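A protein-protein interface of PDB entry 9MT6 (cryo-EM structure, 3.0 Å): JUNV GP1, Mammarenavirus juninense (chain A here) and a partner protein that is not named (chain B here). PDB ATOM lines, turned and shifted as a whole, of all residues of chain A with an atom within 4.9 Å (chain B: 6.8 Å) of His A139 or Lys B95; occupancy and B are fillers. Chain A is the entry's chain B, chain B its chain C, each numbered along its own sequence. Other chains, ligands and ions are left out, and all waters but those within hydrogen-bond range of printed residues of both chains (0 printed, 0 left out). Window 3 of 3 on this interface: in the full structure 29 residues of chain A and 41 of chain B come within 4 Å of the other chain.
A ring nitrogen (NE2) of His A140 sits close to the side-chain sulfur (SD) of Met B92 (3.4 Å). NE of Arg A143 is in hydrogen-bond range of OH of Tyr B104, at 3.2 Å. The backbone carbonyl oxygen (O) of His A139 sits at hydrogen-bond distance from the side-chain amino group (NZ) of Lys B95 (3.2 Å).
Of the 13 printed residues of chain B, 5 touch a printed residue of chain A. Hydrophobic or aromatic side chains of chain A that line the printed part of chain B: His A139, His A140 and His A177.
The side-chain amino group of Lys A135 lies within hydrogen-bond range of a ring nitrogen (NE2) of His A139 (2.9 Å). A ring nitrogen (ND1) of His A140 lies within hydrogen-bond range of the backbone carbonyl oxygen (O) of Thr A136.
Among the printed residues, merely in contact across the chains: Arg A143 with Lys B95, His A177 with Lys B95, His A177 with Leu B91, His A140 with Lys B95 and His A139 with Leu B99.
Of chain B, only Lys B95 and Leu B99 come within 4 Å of His A139. Printed residues of chain A within 4 Å of Lys B95: His A139, His A140, Arg A143 and His A177. Printed residues of chain B within 4 Å of Arg A143: Lys B95 (3.3 Å) and Tyr B104 (3.2 Å). Printed residues of chain B within 4 Å of His A140: Met B92 (3.4 Å) and Lys B95 (3.8 Å). The nearest residue of chain B that does not touch His A139 is Glu B98 (6.7 Å). The nearest printed residue of chain A that does not touch Lys B95 is Tyr A142 (4.001 Å).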
ATOM      1  N   LYS A 135      14.913  18.657  13.148  1.00  0.00           N
ATOM      2  CA  LYS A 135      15.481  18.210  14.414  1.00  0.00           C
ATOM      3  C   LYS A 135      16.437  17.041  14.205  1.00  0.00           C
ATOM      4  O   LYS A 135      17.500  16.977  14.836  1.00  0.00           O
ATOM      5  CB  LYS A 135      14.354  17.837  15.376  1.00  0.00           C
ATOM      6  CG  LYS A 135      14.799  17.281  16.712  1.00  0.00           C
ATOM      7  CD  LYS A 135      13.599  16.810  17.519  1.00  0.00           C
ATOM      8  CE  LYS A 135      14.004  16.332  18.902  1.00  0.00           C
ATOM      9  NZ  LYS A 135      14.841  17.330  19.618  1.00  0.00           N
ATOM     10  N   THR A 136      16.075  16.108  13.321  1.00  0.00           N
ATOM     11  CA  THR A 136      16.991  15.035  12.940  1.00  0.00           C
ATOM     12  C   THR A 136      18.305  15.601  12.427  1.00  0.00           C
ATOM     13  O   THR A 136      19.393  15.202  12.868  1.00  0.00           O
ATOM     14  CB  THR A 136      16.356  14.159  11.862  1.00  0.00           C
ATOM     15  OG1 THR A 136      15.079  13.683  12.296  1.00  0.00           O
ATOM     16  CG2 THR A 136      17.256  12.982  11.536  1.00  0.00           C
ATOM     17  N   GLY A 137      18.217  16.533  11.480  1.00  0.00           N
ATOM     18  CA  GLY A 137      19.416  17.114  10.914  1.00  0.00           C
ATOM     19  C   GLY A 137      20.259  17.826  11.949  1.00  0.00           C
ATOM     20  O   GLY A 137      21.485  17.723  11.938  1.00  0.00           O
ATOM     21  N   MET A 138      19.616  18.552  12.861  1.00  0.00           N
ATOM     22  CA  MET A 138      20.378  19.302  13.853  1.00  0.00           C
ATOM     23  C   MET A 138      21.022  18.386  14.887  1.00  0.00           C
ATOM     24  O   MET A 138      22.109  18.695  15.386  1.00  0.00           O
ATOM     25  CB  MET A 138      19.486  20.341  14.529  1.00  0.00           C
ATOM     26  CG  MET A 138      19.013  21.427  13.586  1.00  0.00           C
ATOM     27  SD  MET A 138      20.290  22.631  13.205  1.00  0.00           S
ATOM     28  CE  MET A 138      21.011  22.878  14.819  1.00  0.00           C
ATOM     29  N   HIS A 139      20.377  17.267  15.229  1.00  0.00           N
ATOM     30  CA  HIS A 139      21.051  16.281  16.067  1.00  0.00           C
ATOM     31  C   HIS A 139      22.236  15.663  15.344  1.00  0.00           C
ATOM     32  O   HIS A 139      23.270  15.383  15.963  1.00  0.00           O
ATOM     33  CB  HIS A 139      20.087  15.191  16.528  1.00  0.00           C
ATOM     34  CG  HIS A 139      19.130  15.638  17.586  1.00  0.00           C
ATOM     35  ND1 HIS A 139      19.526  15.891  18.881  1.00  0.00           N
ATOM     36  CD2 HIS A 139      17.794  15.843  17.555  1.00  0.00           C
ATOM     37  CE1 HIS A 139      18.478  16.255  19.597  1.00  0.00           C
ATOM     38  NE2 HIS A 139      17.414  16.233  18.816  1.00  0.00           N
ATOM     39  N   HIS A 140      22.109  15.430  14.037  1.00  0.00           N
ATOM     40  CA  HIS A 140      23.246  14.916  13.279  1.00  0.00           C
ATOM     41  C   HIS A 140      24.397  15.915  13.265  1.00  0.00           C
ATOM     42  O   HIS A 140      25.537  15.566  13.590  1.00  0.00           O
ATOM     43  CB  HIS A 140      22.826  14.571  11.856  1.00  0.00           C
ATOM     44  CG  HIS A 140      22.405  13.148  11.682  1.00  0.00           C
ATOM     45  ND1 HIS A 140      21.108  12.727  11.870  1.00  0.00           N
ATOM     46  CD2 HIS A 140      23.112  12.048  11.340  1.00  0.00           C
ATOM     47  CE1 HIS A 140      21.033  11.427  11.650  1.00  0.00           C
ATOM     48  NE2 HIS A 140      22.237  10.991  11.327  1.00  0.00           N
ATOM     49  N   LEU A 141      24.115  17.164  12.899  1.00  0.00           N
ATOM     50  CA  LEU A 141      25.172  18.157  12.742  1.00  0.00           C
ATOM     51  C   LEU A 141      25.794  18.536  14.079  1.00  0.00           C
ATOM     52  O   LEU A 141      27.013  18.701  14.179  1.00  0.00           O
ATOM     53  CB  LEU A 141      24.632  19.396  12.026  1.00  0.00           C
ATOM     54  CG  LEU A 141      24.645  19.413  10.494  1.00  0.00           C
ATOM     55  CD1 LEU A 141      23.659  18.442   9.882  1.00  0.00           C
ATOM     56  CD2 LEU A 141      24.359  20.824  10.000  1.00  0.00           C
ATOM     57  N   TYR A 142      24.981  18.686  15.118  1.00  0.00           N
ATOM     58  CA  TYR A 142      25.461  19.106  16.428  1.00  0.00           C
ATOM     59  C   TYR A 142      25.262  17.982  17.434  1.00  0.00           C
ATOM     60  O   TYR A 142      24.135  17.513  17.631  1.00  0.00           O
ATOM     61  CB  TYR A 142      24.736  20.363  16.904  1.00  0.00           C
ATOM     62  CG  TYR A 142      25.054  21.607  16.115  1.00  0.00           C
ATOM     63  CD1 TYR A 142      24.475  21.835  14.877  1.00  0.00           C
ATOM     64  CD2 TYR A 142      25.925  22.559  16.614  1.00  0.00           C
ATOM     65  CE1 TYR A 142      24.759  22.973  14.159  1.00  0.00           C
ATOM     66  CE2 TYR A 142      26.214  23.698  15.902  1.00  0.00           C
ATOM     67  CZ  TYR A 142      25.629  23.901  14.676  1.00  0.00           C
ATOM     68  OH  TYR A 142      25.917  25.038  13.962  1.00  0.00           O
ATOM     69  N   ARG A 143      26.347  17.561  18.078  1.00  0.00           N
ATOM     70  CA  ARG A 143      26.230  16.648  19.202  1.00  0.00           C
ATOM     71  C   ARG A 143      26.005  17.437  20.485  1.00  0.00           C
ATOM     72  O   ARG A 143      26.533  18.538  20.663  1.00  0.00           O
ATOM     73  CB  ARG A 143      27.468  15.759  19.324  1.00  0.00           C
ATOM     74  CG  ARG A 143      28.766  16.491  19.550  1.00  0.00           C
ATOM     75  CD  ARG A 143      29.928  15.512  19.579  1.00  0.00           C
ATOM     76  NE  ARG A 143      30.355  15.218  20.941  1.00  0.00           N
ATOM     77  CZ  ARG A 143      31.157  15.995  21.656  1.00  0.00           C
ATOM     78  NH1 ARG A 143      31.652  17.117  21.162  1.00  0.00           N
ATOM     79  NH2 ARG A 143      31.468  15.638  22.898  1.00  0.00           N
ATOM     80  N   TYR A 145      22.945  18.546  21.118  1.00  0.00           N
ATOM     81  CA  TYR A 145      22.142  19.615  20.533  1.00  0.00           C
ATOM     82  C   TYR A 145      21.091  20.088  21.526  1.00  0.00           C
ATOM     83  O   TYR A 145      20.249  19.288  21.953  1.00  0.00           O
ATOM     84  CB  TYR A 145      21.486  19.123  19.245  1.00  0.00           C
ATOM     85  CG  TYR A 145      20.378  20.003  18.712  1.00  0.00           C
ATOM     86  CD1 TYR A 145      20.549  21.372  18.575  1.00  0.00           C
ATOM     87  CD2 TYR A 145      19.163  19.457  18.331  1.00  0.00           C
ATOM     88  CE1 TYR A 145      19.537  22.170  18.086  1.00  0.00           C
ATOM     89  CE2 TYR A 145      18.147  20.248  17.839  1.00  0.00           C
ATOM     90  CZ  TYR A 145      18.339  21.602  17.721  1.00  0.00           C
ATOM     91  OH  TYR A 145      17.326  22.391  17.231  1.00  0.00           O
ATOM     92  N   ASP A 147      17.919  21.312  21.995  1.00  0.00           N
ATOM     93  CA  ASP A 147      16.644  21.578  21.346  1.00  0.00           C
ATOM     94  C   ASP A 147      15.794  22.511  22.197  1.00  0.00           C
ATOM     95  O   ASP A 147      15.640  22.314  23.405  1.00  0.00           O
ATOM     96  CB  ASP A 147      15.892  20.273  21.086  1.00  0.00           C
ATOM     97  CG  ASP A 147      14.776  20.438  20.073  1.00  0.00           C
ATOM     98  OD1 ASP A 147      14.592  21.563  19.562  1.00  0.00           O
ATOM     99  OD2 ASP A 147      14.079  19.444  19.785  1.00  0.00           O
ATOM    100  N   HIS A 177      29.774  14.678  10.333  1.00  0.00           N
ATOM    101  CA  HIS A 177      28.360  14.527  10.001  1.00  0.00           C
ATOM    102  C   HIS A 177      27.937  15.516   8.922  1.00  0.00           C
ATOM    103  O   HIS A 177      27.164  15.168   8.017  1.00  0.00           O
ATOM    104  CB  HIS A 177      27.505  14.704  11.252  1.00  0.00           C
ATOM    105  CG  HIS A 177      27.395  13.468  12.089  1.00  0.00           C
ATOM    106  ND1 HIS A 177      26.752  12.331  11.653  1.00  0.00           N
ATOM    107  CD2 HIS A 177      27.845  13.191  13.334  1.00  0.00           C
ATOM    108  CE1 HIS A 177      26.811  11.407  12.594  1.00  0.00           C
ATOM    109  NE2 HIS A 177      27.470  11.904  13.624  1.00  0.00           N
ATOM    110  N   LEU B  90      29.699   3.249  11.708  1.00  0.00           N
ATOM    111  CA  LEU B  90      30.180   3.447  13.071  1.00  0.00           C
ATOM    112  C   LEU B  90      29.826   4.832  13.595  1.00  0.00           C
ATOM    113  O   LEU B  90      29.446   4.985  14.762  1.00  0.00           O
ATOM    114  CB  LEU B  90      31.688   3.217  13.127  1.00  0.00           C
ATOM    115  CG  LEU B  90      32.344   3.390  14.492  1.00  0.00           C
ATOM    116  CD1 LEU B  90      31.750   2.424  15.489  1.00  0.00           C
ATOM    117  CD2 LEU B  90      33.841   3.184  14.370  1.00  0.00           C
ATOM    118  N   LEU B  91      29.952   5.852  12.749  1.00  0.00           N
ATOM    119  CA  LEU B  91      29.602   7.205  13.161  1.00  0.00           C
ATOM    120  C   LEU B  91      28.110   7.313  13.460  1.00  0.00           C
ATOM    121  O   LEU B  91      27.706   7.947  14.443  1.00  0.00           O
ATOM    122  CB  LEU B  91      30.028   8.188  12.072  1.00  0.00           C
ATOM    123  CG  LEU B  91      29.906   9.686  12.310  1.00  0.00           C
ATOM    124  CD1 LEU B  91      30.791  10.090  13.465  1.00  0.00           C
ATOM    125  CD2 LEU B  91      30.310  10.426  11.055  1.00  0.00           C
ATOM    126  N   MET B  92      27.278   6.676  12.633  1.00  0.00           N
ATOM    127  CA  MET B  92      25.843   6.648  12.898  1.00  0.00           C
ATOM    128  C   MET B  92      25.534   5.897  14.186  1.00  0.00           C
ATOM    129  O   MET B  92      24.645   6.294  14.947  1.00  0.00           O
ATOM    130  CB  MET B  92      25.105   6.016  11.721  1.00  0.00           C
ATOM    131  CG  MET B  92      23.591   6.065  11.838  1.00  0.00           C
ATOM    132  SD  MET B  92      22.890   7.625  11.270  1.00  0.00           S
ATOM    133  CE  MET B  92      21.613   7.886  12.498  1.00  0.00           C
ATOM    134  N   LYS B  93      26.252   4.801  14.442  1.00  0.00           N
ATOM    135  CA  LYS B  93      26.055   4.056  15.679  1.00  0.00           C
ATOM    136  C   LYS B  93      26.394   4.910  16.891  1.00  0.00           C
ATOM    137  O   LYS B  93      25.675   4.890  17.895  1.00  0.00           O
ATOM    138  CB  LYS B  93      26.905   2.787  15.669  1.00  0.00           C
ATOM    139  CG  LYS B  93      26.642   1.857  16.839  1.00  0.00           C
ATOM    140  CD  LYS B  93      27.309   0.509  16.634  1.00  0.00           C
ATOM    141  CE  LYS B  93      28.797   0.585  16.937  1.00  0.00           C
ATOM    142  NZ  LYS B  93      29.311  -0.685  17.518  1.00  0.00           N
ATOM    143  N   ASN B  94      27.487   5.668  16.814  1.00  0.00           N
ATOM    144  CA  ASN B  94      27.856   6.544  17.919  1.00  0.00           C
ATOM    145  C   ASN B  94      26.831   7.654  18.111  1.00  0.00           C
ATOM    146  O   ASN B  94      26.522   8.034  19.245  1.00  0.00           O
ATOM    147  CB  ASN B  94      29.247   7.126  17.686  1.00  0.00           C
ATOM    148  CG  ASN B  94      30.344   6.213  18.183  1.00  0.00           C
ATOM    149  OD1 ASN B  94      30.691   6.230  19.361  1.00  0.00           O
ATOM    150  ND2 ASN B  94      30.897   5.409  17.285  1.00  0.00           N
ATOM    151  N   LYS B  95      26.289   8.188  17.012  1.00  0.00           N
ATOM    152  CA  LYS B  95      25.245   9.203  17.135  1.00  0.00           C
ATOM    153  C   LYS B  95      23.991   8.631  17.787  1.00  0.00           C
ATOM    154  O   LYS B  95      23.370   9.278  18.641  1.00  0.00           O
ATOM    155  CB  LYS B  95      24.922   9.792  15.763  1.00  0.00           C
ATOM    156  CG  LYS B  95      23.896  10.911  15.792  1.00  0.00           C
ATOM    157  CD  LYS B  95      24.282  11.972  16.802  1.00  0.00           C
ATOM    158  CE  LYS B  95      25.325  12.908  16.245  1.00  0.00           C
ATOM    159  NZ  LYS B  95      25.769  13.879  17.268  1.00  0.00           N
ATOM    160  N   ILE B  96      23.610   7.410  17.405  1.00  0.00           N
ATOM    161  CA  ILE B  96      22.448   6.767  18.012  1.00  0.00           C
ATOM    162  C   ILE B  96      22.694   6.510  19.491  1.00  0.00           C
ATOM    163  O   ILE B  96      21.795   6.681  20.323  1.00  0.00           O
ATOM    164  CB  ILE B  96      22.096   5.472  17.258  1.00  0.00           C
ATOM    165  CG1 ILE B  96      21.631   5.789  15.838  1.00  0.00           C
ATOM    166  CG2 ILE B  96      21.028   4.691  18.001  1.00  0.00           C
ATOM    167  CD1 ILE B  96      21.504   4.569  14.959  1.00  0.00           C
ATOM    168  N   ARG B  97      23.909   6.086  19.845  1.00  0.00           N
ATOM    169  CA  ARG B  97      24.240   5.874  21.251  1.00  0.00           C
ATOM    170  C   ARG B  97      24.179   7.178  22.036  1.00  0.00           C
ATOM    171  O   ARG B  97      23.736   7.196  23.190  1.00  0.00           O
ATOM    172  CB  ARG B  97      25.623   5.235  21.374  1.00  0.00           C
ATOM    173  CG  ARG B  97      25.681   3.799  20.895  1.00  0.00           C
ATOM    174  CD  ARG B  97      26.625   2.973  21.743  1.00  0.00           C
ATOM    175  NE  ARG B  97      28.021   3.266  21.445  1.00  0.00           N
ATOM    176  CZ  ARG B  97      28.804   2.492  20.705  1.00  0.00           C
ATOM    177  NH1 ARG B  97      28.358   1.367  20.170  1.00  0.00           N
ATOM    178  NH2 ARG B  97      30.066   2.856  20.499  1.00  0.00           N
ATOM    179  N   GLU B  98      24.635   8.277  21.434  1.00  0.00           N
ATOM    180  CA  GLU B  98      24.512   9.581  22.076  1.00  0.00           C
ATOM    181  C   GLU B  98      23.053   9.942  22.306  1.00  0.00           C
ATOM    182  O   GLU B  98      22.696  10.473  23.364  1.00  0.00           O
ATOM    183  CB  GLU B  98      25.200  10.651  21.225  1.00  0.00           C
ATOM    184  CG  GLU B  98      24.882  12.119  21.557  1.00  0.00           C
ATOM    185  CD  GLU B  98      25.036  12.524  23.027  1.00  0.00           C
ATOM    186  OE1 GLU B  98      25.454  11.708  23.872  1.00  0.00           O
ATOM    187  OE2 GLU B  98      24.726  13.695  23.338  1.00  0.00           O
ATOM    188  N   LEU B  99      22.195   9.667  21.324  1.00  0.00           N
ATOM    189  CA  LEU B  99      20.775   9.969  21.487  1.00  0.00           C
ATOM    190  C   LEU B  99      20.139   9.088  22.557  1.00  0.00           C
ATOM    191  O   LEU B  99      19.254   9.536  23.295  1.00  0.00           O
ATOM    192  CB  LEU B  99      20.053   9.814  20.153  1.00  0.00           C
ATOM    193  CG  LEU B  99      20.496  10.826  19.098  1.00  0.00           C
ATOM    194  CD1 LEU B  99      19.841  10.531  17.768  1.00  0.00           C
ATOM    195  CD2 LEU B  99      20.190  12.243  19.551  1.00  0.00           C
ATOM    196  N   MET B 100      20.580   7.833  22.661  1.00  0.00           N
ATOM    197  CA  MET B 100      20.086   6.915  23.678  1.00  0.00           C
ATOM    198  C   MET B 100      20.594   7.248  25.073  1.00  0.00           C
ATOM    199  O   MET B 100      20.136   6.632  26.039  1.00  0.00           O
ATOM    200  CB  MET B 100      20.484   5.479  23.335  1.00  0.00           C
ATOM    201  CG  MET B 100      19.827   4.914  22.094  1.00  0.00           C
ATOM    202  SD  MET B 100      19.596   3.133  22.200  1.00  0.00           S
ATOM    203  CE  MET B 100      18.775   2.802  20.644  1.00  0.00           C
ATOM    204  N   TYR B 104      29.242   6.688  24.430  1.00  0.00           N
ATOM    205  CA  TYR B 104      29.592   6.768  23.020  1.00  0.00           C
ATOM    206  C   TYR B 104      31.021   7.276  22.902  1.00  0.00           C
ATOM    207  O   TYR B 104      31.700   7.521  23.901  1.00  0.00           O
ATOM    208  CB  TYR B 104      28.605   7.658  22.253  1.00  0.00           C
ATOM    209  CG  TYR B 104      28.770   9.143  22.497  1.00  0.00           C
ATOM    210  CD1 TYR B 104      28.307   9.729  23.666  1.00  0.00           C
ATOM    211  CD2 TYR B 104      29.378   9.958  21.556  1.00  0.00           C
ATOM    212  CE1 TYR B 104      28.452  11.081  23.890  1.00  0.00           C
ATOM    213  CE2 TYR B 104      29.530  11.310  21.775  1.00  0.00           C
ATOM    214  CZ  TYR B 104      29.065  11.865  22.943  1.00  0.00           C
ATOM    215  OH  TYR B 104      29.212  13.213  23.165  1.00  0.00           O
ATOM    216  N   CYS B 105      31.483   7.430  21.665  1.00  0.00           N
ATOM    217  CA  CYS B 105      32.849   7.837  21.372  1.00  0.00           C
ATOM    218  C   CYS B 105      32.825   9.120  20.556  1.00  0.00           C
ATOM    219  O   CYS B 105      32.144   9.189  19.528  1.00  0.00           O
ATOM    220  CB  CYS B 105      33.585   6.734  20.608  1.00  0.00           C
ATOM    221  SG  CYS B 105      35.293   7.096  20.186  1.00  0.00           S
